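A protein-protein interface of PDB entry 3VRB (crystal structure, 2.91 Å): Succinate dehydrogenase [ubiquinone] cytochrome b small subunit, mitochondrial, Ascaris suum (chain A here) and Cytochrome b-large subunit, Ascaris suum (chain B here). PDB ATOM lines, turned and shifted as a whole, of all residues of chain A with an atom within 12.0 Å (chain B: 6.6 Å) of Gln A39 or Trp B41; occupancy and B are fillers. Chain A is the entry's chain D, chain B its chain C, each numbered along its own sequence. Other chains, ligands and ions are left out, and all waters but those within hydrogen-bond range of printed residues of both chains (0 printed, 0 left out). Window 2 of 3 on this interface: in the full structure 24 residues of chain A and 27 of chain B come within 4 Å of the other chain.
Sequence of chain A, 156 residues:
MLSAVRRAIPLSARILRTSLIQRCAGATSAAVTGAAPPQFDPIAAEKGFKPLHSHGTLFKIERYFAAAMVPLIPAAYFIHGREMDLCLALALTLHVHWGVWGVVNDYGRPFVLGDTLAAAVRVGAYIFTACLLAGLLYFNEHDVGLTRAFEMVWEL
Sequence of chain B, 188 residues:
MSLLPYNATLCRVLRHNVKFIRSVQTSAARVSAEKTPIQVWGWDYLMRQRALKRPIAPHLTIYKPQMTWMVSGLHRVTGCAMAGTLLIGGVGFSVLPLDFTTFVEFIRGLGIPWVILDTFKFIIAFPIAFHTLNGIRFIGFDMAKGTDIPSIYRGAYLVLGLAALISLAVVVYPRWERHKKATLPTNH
Of the 12 printed residues of chain B, 5 touch a printed residue of chain A.
Hydrophobic or aromatic side chains of chain B within 4 Å of the printed part of chain A: Pro B37, Trp B41 and Leu B46.
Hydrophobic or aromatic side chains of chain A within 4 Å of the printed part of chain B: Pro A38, Phe A40, Phe A49 and Phe A111.
Among the printed residues, 7 pairs touch across the chains.
Among the printed residues, no Asp or Glu carboxylate lies within 4 Å of a Lys or Arg side-chain nitrogen of the other chain.
Among the printed residues, merely in contact across the chains: Gln A39 with Trp B41, Phe A111 with Leu B46, Phe A40 with Trp B41, Pro A38 with Arg B48, Phe A49 with Pro B37, Phe A40 with Ile B38 and Phe A40 with Pro B37.
Of chain B, only Trp B41 comes within 4 Å of Gln A39.
Of the printed residues of chain B, Phe A40 touches Pro B37 (3.9 Å), Ile B38 (3.9 Å) and Trp B41 (3.7 Å).
Of the printed residues of chain B, Phe A49 touches Pro B37 (3.9 Å).
Of the printed residues of chain B, Phe A111 touches Leu B46 (3.6 Å).
Trp B41 touches two residues of chain A.
No residue of chain A comes within 4 Å of Gly B42.
No residue of chain A comes within 4 Å of Asp B44.
The nearest printed residue of chain A that does not touch Leu B46 is Pro A38 (9.8 Å).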
ATOM      1  N   ALA A  35      11.645  30.080 -30.453  1.00  0.00           N
ATOM      2  CA  ALA A  35      11.040  30.912 -29.410  1.00  0.00           C
ATOM      3  C   ALA A  35      12.001  31.359 -28.298  1.00  0.00           C
ATOM      4  O   ALA A  35      13.190  30.984 -28.249  1.00  0.00           O
ATOM      5  CB  ALA A  35       9.805  30.215 -28.796  1.00  0.00           C
ATOM      6  N   ALA A  36      11.422  32.166 -27.409  1.00  0.00           N
ATOM      7  CA  ALA A  36      12.076  32.744 -26.237  1.00  0.00           C
ATOM      8  C   ALA A  36      12.118  31.719 -25.124  1.00  0.00           C
ATOM      9  O   ALA A  36      11.068  31.323 -24.637  1.00  0.00           O
ATOM     10  CB  ALA A  36      11.292  33.981 -25.771  1.00  0.00           C
ATOM     11  N   PRO A  37      13.324  31.286 -24.715  1.00  0.00           N
ATOM     12  CA  PRO A  37      13.457  30.258 -23.666  1.00  0.00           C
ATOM     13  C   PRO A  37      12.588  30.469 -22.401  1.00  0.00           C
ATOM     14  O   PRO A  37      12.487  31.600 -21.901  1.00  0.00           O
ATOM     15  CB  PRO A  37      14.957  30.290 -23.338  1.00  0.00           C
ATOM     16  CG  PRO A  37      15.601  30.636 -24.642  1.00  0.00           C
ATOM     17  CD  PRO A  37      14.626  31.592 -25.347  1.00  0.00           C
ATOM     18  N   PRO A  38      11.943  29.378 -21.912  1.00  0.00           N
ATOM     19  CA  PRO A  38      11.096  29.357 -20.726  1.00  0.00           C
ATOM     20  C   PRO A  38      11.596  30.287 -19.631  1.00  0.00           C
ATOM     21  O   PRO A  38      12.750  30.200 -19.234  1.00  0.00           O
ATOM     22  CB  PRO A  38      11.188  27.899 -20.273  1.00  0.00           C
ATOM     23  CG  PRO A  38      11.593  27.102 -21.524  1.00  0.00           C
ATOM     24  CD  PRO A  38      11.892  28.077 -22.610  1.00  0.00           C
ATOM     25  N   GLN A  39      10.731  31.184 -19.180  1.00  0.00           N
ATOM     26  CA  GLN A  39      11.076  32.169 -18.165  1.00  0.00           C
ATOM     27  C   GLN A  39       9.840  32.421 -17.323  1.00  0.00           C
ATOM     28  O   GLN A  39       8.717  32.242 -17.794  1.00  0.00           O
ATOM     29  CB  GLN A  39      11.562  33.475 -18.827  1.00  0.00           C
ATOM     30  CG  GLN A  39      11.699  34.690 -17.861  1.00  0.00           C
ATOM     31  CD  GLN A  39      12.368  35.939 -18.463  1.00  0.00           C
ATOM     32  OE1 GLN A  39      12.184  36.278 -19.634  1.00  0.00           O
ATOM     33  NE2 GLN A  39      13.127  36.640 -17.636  1.00  0.00           N
ATOM     34  N   PHE A  40      10.029  32.832 -16.080  1.00  0.00           N
ATOM     35  CA  PHE A  40       8.888  33.192 -15.273  1.00  0.00           C
ATOM     36  C   PHE A  40       8.718  34.681 -15.241  1.00  0.00           C
ATOM     37  O   PHE A  40       9.656  35.410 -14.946  1.00  0.00           O
ATOM     38  CB  PHE A  40       9.040  32.665 -13.869  1.00  0.00           C
ATOM     39  CG  PHE A  40       7.808  32.792 -13.043  1.00  0.00           C
ATOM     40  CD1 PHE A  40       6.708  31.987 -13.291  1.00  0.00           C
ATOM     41  CD2 PHE A  40       7.758  33.692 -11.987  1.00  0.00           C
ATOM     42  CE1 PHE A  40       5.563  32.092 -12.509  1.00  0.00           C
ATOM     43  CE2 PHE A  40       6.618  33.806 -11.195  1.00  0.00           C
ATOM     44  CZ  PHE A  40       5.516  33.005 -11.457  1.00  0.00           C
ATOM     45  N   ASP A  41       7.509  35.125 -15.561  1.00  0.00           N
ATOM     46  CA  ASP A  41       7.160  36.534 -15.472  1.00  0.00           C
ATOM     47  C   ASP A  41       6.185  36.773 -14.318  1.00  0.00           C
ATOM     48  O   ASP A  41       5.002  36.474 -14.420  1.00  0.00           O
ATOM     49  CB  ASP A  41       6.581  37.021 -16.791  1.00  0.00           C
ATOM     50  CG  ASP A  41       6.534  38.539 -16.884  1.00  0.00           C
ATOM     51  OD1 ASP A  41       5.687  39.154 -16.185  1.00  0.00           O
ATOM     52  OD2 ASP A  41       7.336  39.114 -17.671  1.00  0.00           O
ATOM     53  N   PRO A  42       6.688  37.328 -13.216  1.00  0.00           N
ATOM     54  CA  PRO A  42       5.978  37.385 -11.950  1.00  0.00           C
ATOM     55  C   PRO A  42       4.808  38.341 -11.947  1.00  0.00           C
ATOM     56  O   PRO A  42       3.991  38.299 -11.026  1.00  0.00           O
ATOM     57  CB  PRO A  42       7.043  37.895 -10.985  1.00  0.00           C
ATOM     58  CG  PRO A  42       7.931  38.691 -11.825  1.00  0.00           C
ATOM     59  CD  PRO A  42       7.984  38.014 -13.149  1.00  0.00           C
ATOM     60  N   ILE A  43       4.744  39.208 -12.954  1.00  0.00           N
ATOM     61  CA  ILE A  43       3.706  40.243 -13.027  1.00  0.00           C
ATOM     62  C   ILE A  43       2.543  39.837 -13.944  1.00  0.00           C
ATOM     63  O   ILE A  43       1.369  40.106 -13.649  1.00  0.00           O
ATOM     64  CB  ILE A  43       4.312  41.647 -13.371  1.00  0.00           C
ATOM     65  CG1 ILE A  43       4.392  42.485 -12.079  1.00  0.00           C
ATOM     66  CG2 ILE A  43       3.549  42.327 -14.507  1.00  0.00           C
ATOM     67  CD1 ILE A  43       3.623  43.810 -12.070  1.00  0.00           C
ATOM     68  N   ALA A  44       2.899  39.172 -15.039  1.00  0.00           N
ATOM     69  CA  ALA A  44       1.944  38.559 -15.946  1.00  0.00           C
ATOM     70  C   ALA A  44       1.284  37.354 -15.286  1.00  0.00           C
ATOM     71  O   ALA A  44       0.298  36.819 -15.788  1.00  0.00           O
ATOM     72  CB  ALA A  44       2.643  38.144 -17.237  1.00  0.00           C
ATOM     73  N   ALA A  45       1.830  36.930 -14.158  1.00  0.00           N
ATOM     74  CA  ALA A  45       1.309  35.781 -13.462  1.00  0.00           C
ATOM     75  C   ALA A  45       0.317  36.237 -12.412  1.00  0.00           C
ATOM     76  O   ALA A  45      -0.619  35.516 -12.078  1.00  0.00           O
ATOM     77  CB  ALA A  45       2.432  35.018 -12.834  1.00  0.00           C
ATOM     78  N   GLU A  46       0.522  37.450 -11.911  1.00  0.00           N
ATOM     79  CA  GLU A  46      -0.334  38.035 -10.879  1.00  0.00           C
ATOM     80  C   GLU A  46      -1.772  38.302 -11.352  1.00  0.00           C
ATOM     81  O   GLU A  46      -2.630  38.681 -10.541  1.00  0.00           O
ATOM     82  CB  GLU A  46       0.304  39.325 -10.347  1.00  0.00           C
ATOM     83  CG  GLU A  46      -0.361  39.897  -9.097  1.00  0.00           C
ATOM     84  CD  GLU A  46       0.639  40.519  -8.139  1.00  0.00           C
ATOM     85  OE1 GLU A  46       1.414  41.411  -8.564  1.00  0.00           O
ATOM     86  OE2 GLU A  46       0.647  40.106  -6.957  1.00  0.00           O
ATOM     87  N   PHE A  49      -5.175  35.168  -9.918  1.00  0.00           N
ATOM     88  CA  PHE A  49      -4.591  34.301  -8.859  1.00  0.00           C
ATOM     89  C   PHE A  49      -4.369  35.064  -7.529  1.00  0.00           C
ATOM     90  O   PHE A  49      -3.359  35.772  -7.375  1.00  0.00           O
ATOM     91  CB  PHE A  49      -3.238  33.705  -9.315  1.00  0.00           C
ATOM     92  CG  PHE A  49      -3.264  32.211  -9.636  1.00  0.00           C
ATOM     93  CD1 PHE A  49      -3.658  31.266  -8.674  1.00  0.00           C
ATOM     94  CD2 PHE A  49      -2.819  31.744 -10.887  1.00  0.00           C
ATOM     95  CE1 PHE A  49      -3.651  29.878  -8.978  1.00  0.00           C
ATOM     96  CE2 PHE A  49      -2.799  30.362 -11.198  1.00  0.00           C
ATOM     97  CZ  PHE A  49      -3.216  29.432 -10.247  1.00  0.00           C
ATOM     98  N   PHE A 111       6.286  13.858  -8.151  1.00  0.00           N
ATOM     99  CA  PHE A 111       7.360  13.688  -9.139  1.00  0.00           C
ATOM    100  C   PHE A 111       7.873  12.250  -9.187  1.00  0.00           C
ATOM    101  O   PHE A 111       8.068  11.686 -10.262  1.00  0.00           O
ATOM    102  CB  PHE A 111       8.521  14.664  -8.923  1.00  0.00           C
ATOM    103  CG  PHE A 111       9.552  14.635 -10.040  1.00  0.00           C
ATOM    104  CD1 PHE A 111       9.257  15.160 -11.298  1.00  0.00           C
ATOM    105  CD2 PHE A 111      10.815  14.071  -9.836  1.00  0.00           C
ATOM    106  CE1 PHE A 111      10.199  15.123 -12.323  1.00  0.00           C
ATOM    107  CE2 PHE A 111      11.770  14.037 -10.865  1.00  0.00           C
ATOM    108  CZ  PHE A 111      11.458  14.562 -12.106  1.00  0.00           C
ATOM    109  N   THR B  36       0.161  27.975  -6.197  1.00  0.00           N
ATOM    110  CA  THR B  36       0.499  29.320  -6.658  1.00  0.00           C
ATOM    111  C   THR B  36       1.112  29.233  -8.065  1.00  0.00           C
ATOM    112  O   THR B  36       1.706  28.208  -8.423  1.00  0.00           O
ATOM    113  CB  THR B  36       1.491  29.986  -5.719  1.00  0.00           C
ATOM    114  OG1 THR B  36       2.656  29.156  -5.608  1.00  0.00           O
ATOM    115  CG2 THR B  36       0.862  30.189  -4.344  1.00  0.00           C
ATOM    116  N   PRO B  37       0.979  30.305  -8.869  1.00  0.00           N
ATOM    117  CA  PRO B  37       1.478  30.307 -10.261  1.00  0.00           C
ATOM    118  C   PRO B  37       2.921  29.789 -10.430  1.00  0.00           C
ATOM    119  O   PRO B  37       3.219  29.116 -11.412  1.00  0.00           O
ATOM    120  CB  PRO B  37       1.368  31.785 -10.677  1.00  0.00           C
ATOM    121  CG  PRO B  37       1.072  32.559  -9.402  1.00  0.00           C
ATOM    122  CD  PRO B  37       0.392  31.604  -8.487  1.00  0.00           C
ATOM    123  N   ILE B  38       3.787  30.106  -9.472  1.00  0.00           N
ATOM    124  CA  ILE B  38       5.176  29.637  -9.463  1.00  0.00           C
ATOM    125  C   ILE B  38       5.316  28.106  -9.300  1.00  0.00           C
ATOM    126  O   ILE B  38       6.101  27.457  -9.995  1.00  0.00           O
ATOM    127  CB  ILE B  38       6.021  30.412  -8.384  1.00  0.00           C
ATOM    128  CG1 ILE B  38       7.494  29.991  -8.418  1.00  0.00           C
ATOM    129  CG2 ILE B  38       5.397  30.298  -6.960  1.00  0.00           C
ATOM    130  CD1 ILE B  38       8.216  30.412  -9.672  1.00  0.00           C
ATOM    131  N   GLN B  39       4.547  27.548  -8.373  1.00  0.00           N
ATOM    132  CA  GLN B  39       4.477  26.104  -8.192  1.00  0.00           C
ATOM    133  C   GLN B  39       4.093  25.420  -9.489  1.00  0.00           C
ATOM    134  O   GLN B  39       4.557  24.327  -9.792  1.00  0.00           O
ATOM    135  CB  GLN B  39       3.494  25.747  -7.082  1.00  0.00           C
ATOM    136  CG  GLN B  39       3.875  26.400  -5.785  1.00  0.00           C
ATOM    137  CD  GLN B  39       2.963  26.037  -4.639  1.00  0.00           C
ATOM    138  OE1 GLN B  39       1.741  26.188  -4.720  1.00  0.00           O
ATOM    139  NE2 GLN B  39       3.560  25.582  -3.536  1.00  0.00           N
ATOM    140  N   VAL B  40       3.258  26.077 -10.268  1.00  0.00           N
ATOM    141  CA  VAL B  40       2.884  25.514 -11.524  1.00  0.00           C
ATOM    142  C   VAL B  40       4.108  25.517 -12.417  1.00  0.00           C
ATOM    143  O   VAL B  40       4.404  24.517 -13.080  1.00  0.00           O
ATOM    144  CB  VAL B  40       1.773  26.314 -12.165  1.00  0.00           C
ATOM    145  CG1 VAL B  40       1.101  25.497 -13.270  1.00  0.00           C
ATOM    146  CG2 VAL B  40       0.792  26.714 -11.114  1.00  0.00           C
ATOM    147  N   TRP B  41       4.825  26.639 -12.415  1.00  0.00           N
ATOM    148  CA  TRP B  41       5.985  26.784 -13.270  1.00  0.00           C
ATOM    149  C   TRP B  41       6.995  25.683 -12.904  1.00  0.00           C
ATOM    150  O   TRP B  41       7.594  25.027 -13.781  1.00  0.00           O
ATOM    151  CB  TRP B  41       6.593  28.193 -13.135  1.00  0.00           C
ATOM    152  CG  TRP B  41       7.523  28.471 -14.241  1.00  0.00           C
ATOM    153  CD1 TRP B  41       7.196  28.989 -15.431  1.00  0.00           C
ATOM    154  CD2 TRP B  41       8.939  28.189 -14.298  1.00  0.00           C
ATOM    155  NE1 TRP B  41       8.308  29.084 -16.233  1.00  0.00           N
ATOM    156  CE2 TRP B  41       9.390  28.593 -15.563  1.00  0.00           C
ATOM    157  CE3 TRP B  41       9.868  27.653 -13.391  1.00  0.00           C
ATOM    158  CZ2 TRP B  41      10.715  28.471 -15.966  1.00  0.00           C
ATOM    159  CZ3 TRP B  41      11.211  27.528 -13.794  1.00  0.00           C
ATOM    160  CH2 TRP B  41      11.613  27.934 -15.071  1.00  0.00           C
ATOM    161  N   GLY B  42       7.135  25.482 -11.592  1.00  0.00           N
ATOM    162  CA  GLY B  42       8.048  24.514 -11.024  1.00  0.00           C
ATOM    163  C   GLY B  42       7.763  23.127 -11.534  1.00  0.00           C
ATOM    164  O   GLY B  42       8.675  22.379 -11.885  1.00  0.00           O
ATOM    165  N   TRP B  43       6.483  22.782 -11.573  1.00  0.00           N
ATOM    166  CA  TRP B  43       6.084  21.500 -12.104  1.00  0.00           C
ATOM    167  C   TRP B  43       6.639  21.313 -13.530  1.00  0.00           C
ATOM    168  O   TRP B  43       7.415  20.382 -13.790  1.00  0.00           O
ATOM    169  CB  TRP B  43       4.558  21.317 -12.050  1.00  0.00           C
ATOM    170  CG  TRP B  43       4.170  19.928 -12.516  1.00  0.00           C
ATOM    171  CD1 TRP B  43       3.605  19.580 -13.725  1.00  0.00           C
ATOM    172  CD2 TRP B  43       4.385  18.704 -11.813  1.00  0.00           C
ATOM    173  NE1 TRP B  43       3.446  18.226 -13.794  1.00  0.00           N
ATOM    174  CE2 TRP B  43       3.922  17.666 -12.633  1.00  0.00           C
ATOM    175  CE3 TRP B  43       4.921  18.386 -10.561  1.00  0.00           C
ATOM    176  CZ2 TRP B  43       3.972  16.331 -12.235  1.00  0.00           C
ATOM    177  CZ3 TRP B  43       4.970  17.061 -10.172  1.00  0.00           C
ATOM    178  CH2 TRP B  43       4.502  16.055 -11.004  1.00  0.00           C
ATOM    179  N   ASP B  44       6.277  22.219 -14.434  1.00  0.00           N
ATOM    180  CA  ASP B  44       6.641  22.071 -15.837  1.00  0.00           C
ATOM    181  C   ASP B  44       8.133  21.989 -15.939  1.00  0.00           C
ATOM    182  O   ASP B  44       8.660  21.288 -16.798  1.00  0.00           O
ATOM    183  CB  ASP B  44       6.153  23.250 -16.677  1.00  0.00           C
ATOM    184  CG  ASP B  44       4.699  23.633 -16.394  1.00  0.00           C
ATOM    185  OD1 ASP B  44       4.453  24.847 -16.151  1.00  0.00           O
ATOM    186  OD2 ASP B  44       3.812  22.732 -16.419  1.00  0.00           O
ATOM    187  N   TYR B  45       8.815  22.717 -15.059  1.00  0.00           N
ATOM    188  CA  TYR B  45      10.261  22.698 -15.049  1.00  0.00           C
ATOM    189  C   TYR B  45      10.760  21.270 -14.848  1.00  0.00           C
ATOM    190  O   TYR B  45      11.655  20.797 -15.541  1.00  0.00           O
ATOM    191  CB  TYR B  45      10.832  23.649 -13.989  1.00  0.00           C
ATOM    192  CG  TYR B  45      12.287  23.378 -13.709  1.00  0.00           C
ATOM    193  CD1 TYR B  45      13.269  23.685 -14.643  1.00  0.00           C
ATOM    194  CD2 TYR B  45      12.681  22.763 -12.528  1.00  0.00           C
ATOM    195  CE1 TYR B  45      14.606  23.406 -14.393  1.00  0.00           C
ATOM    196  CE2 TYR B  45      14.016  22.475 -12.278  1.00  0.00           C
ATOM    197  CZ  TYR B  45      14.967  22.801 -13.214  1.00  0.00           C
ATOM    198  OH  TYR B  45      16.279  22.510 -12.953  1.00  0.00           O
ATOM    199  N   LEU B  46      10.162  20.566 -13.906  1.00  0.00           N
ATOM    200  CA  LEU B  46      10.650  19.242 -13.601  1.00  0.00           C
ATOM    201  C   LEU B  46      10.286  18.336 -14.738  1.00  0.00           C
ATOM    202  O   LEU B  46      11.085  17.507 -15.133  1.00  0.00           O
ATOM    203  CB  LEU B  46      10.136  18.740 -12.249  1.00  0.00           C
ATOM    204  CG  LEU B  46      10.562  19.520 -10.978  1.00  0.00           C
ATOM    205  CD1 LEU B  46       9.774  19.041  -9.778  1.00  0.00           C
ATOM    206  CD2 LEU B  46      12.050  19.459 -10.646  1.00  0.00           C
ATOM    207  N   ARG B  48      10.085  19.273 -17.925  1.00  0.00           N
ATOM    208  CA  ARG B  48      11.133  19.625 -18.860  1.00  0.00           C
ATOM    209  C   ARG B  48      12.455  18.905 -18.529  1.00  0.00           C
ATOM    210  O   ARG B  48      13.115  18.343 -19.415  1.00  0.00           O
ATOM    211  CB  ARG B  48      11.321  21.142 -18.883  1.00  0.00           C
ATOM    212  CG  ARG B  48      10.487  21.840 -19.935  1.00  0.00           C
ATOM    213  CD  ARG B  48      10.802  23.317 -20.035  1.00  0.00           C
ATOM    214  NE  ARG B  48       9.975  24.121 -19.133  1.00  0.00           N
ATOM    215  CZ  ARG B  48      10.442  24.859 -18.123  1.00  0.00           C
ATOM    216  NH1 ARG B  48      11.754  24.897 -17.870  1.00  0.00           N
ATOM    217  NH2 ARG B  48       9.595  25.569 -17.368  1.00  0.00           N
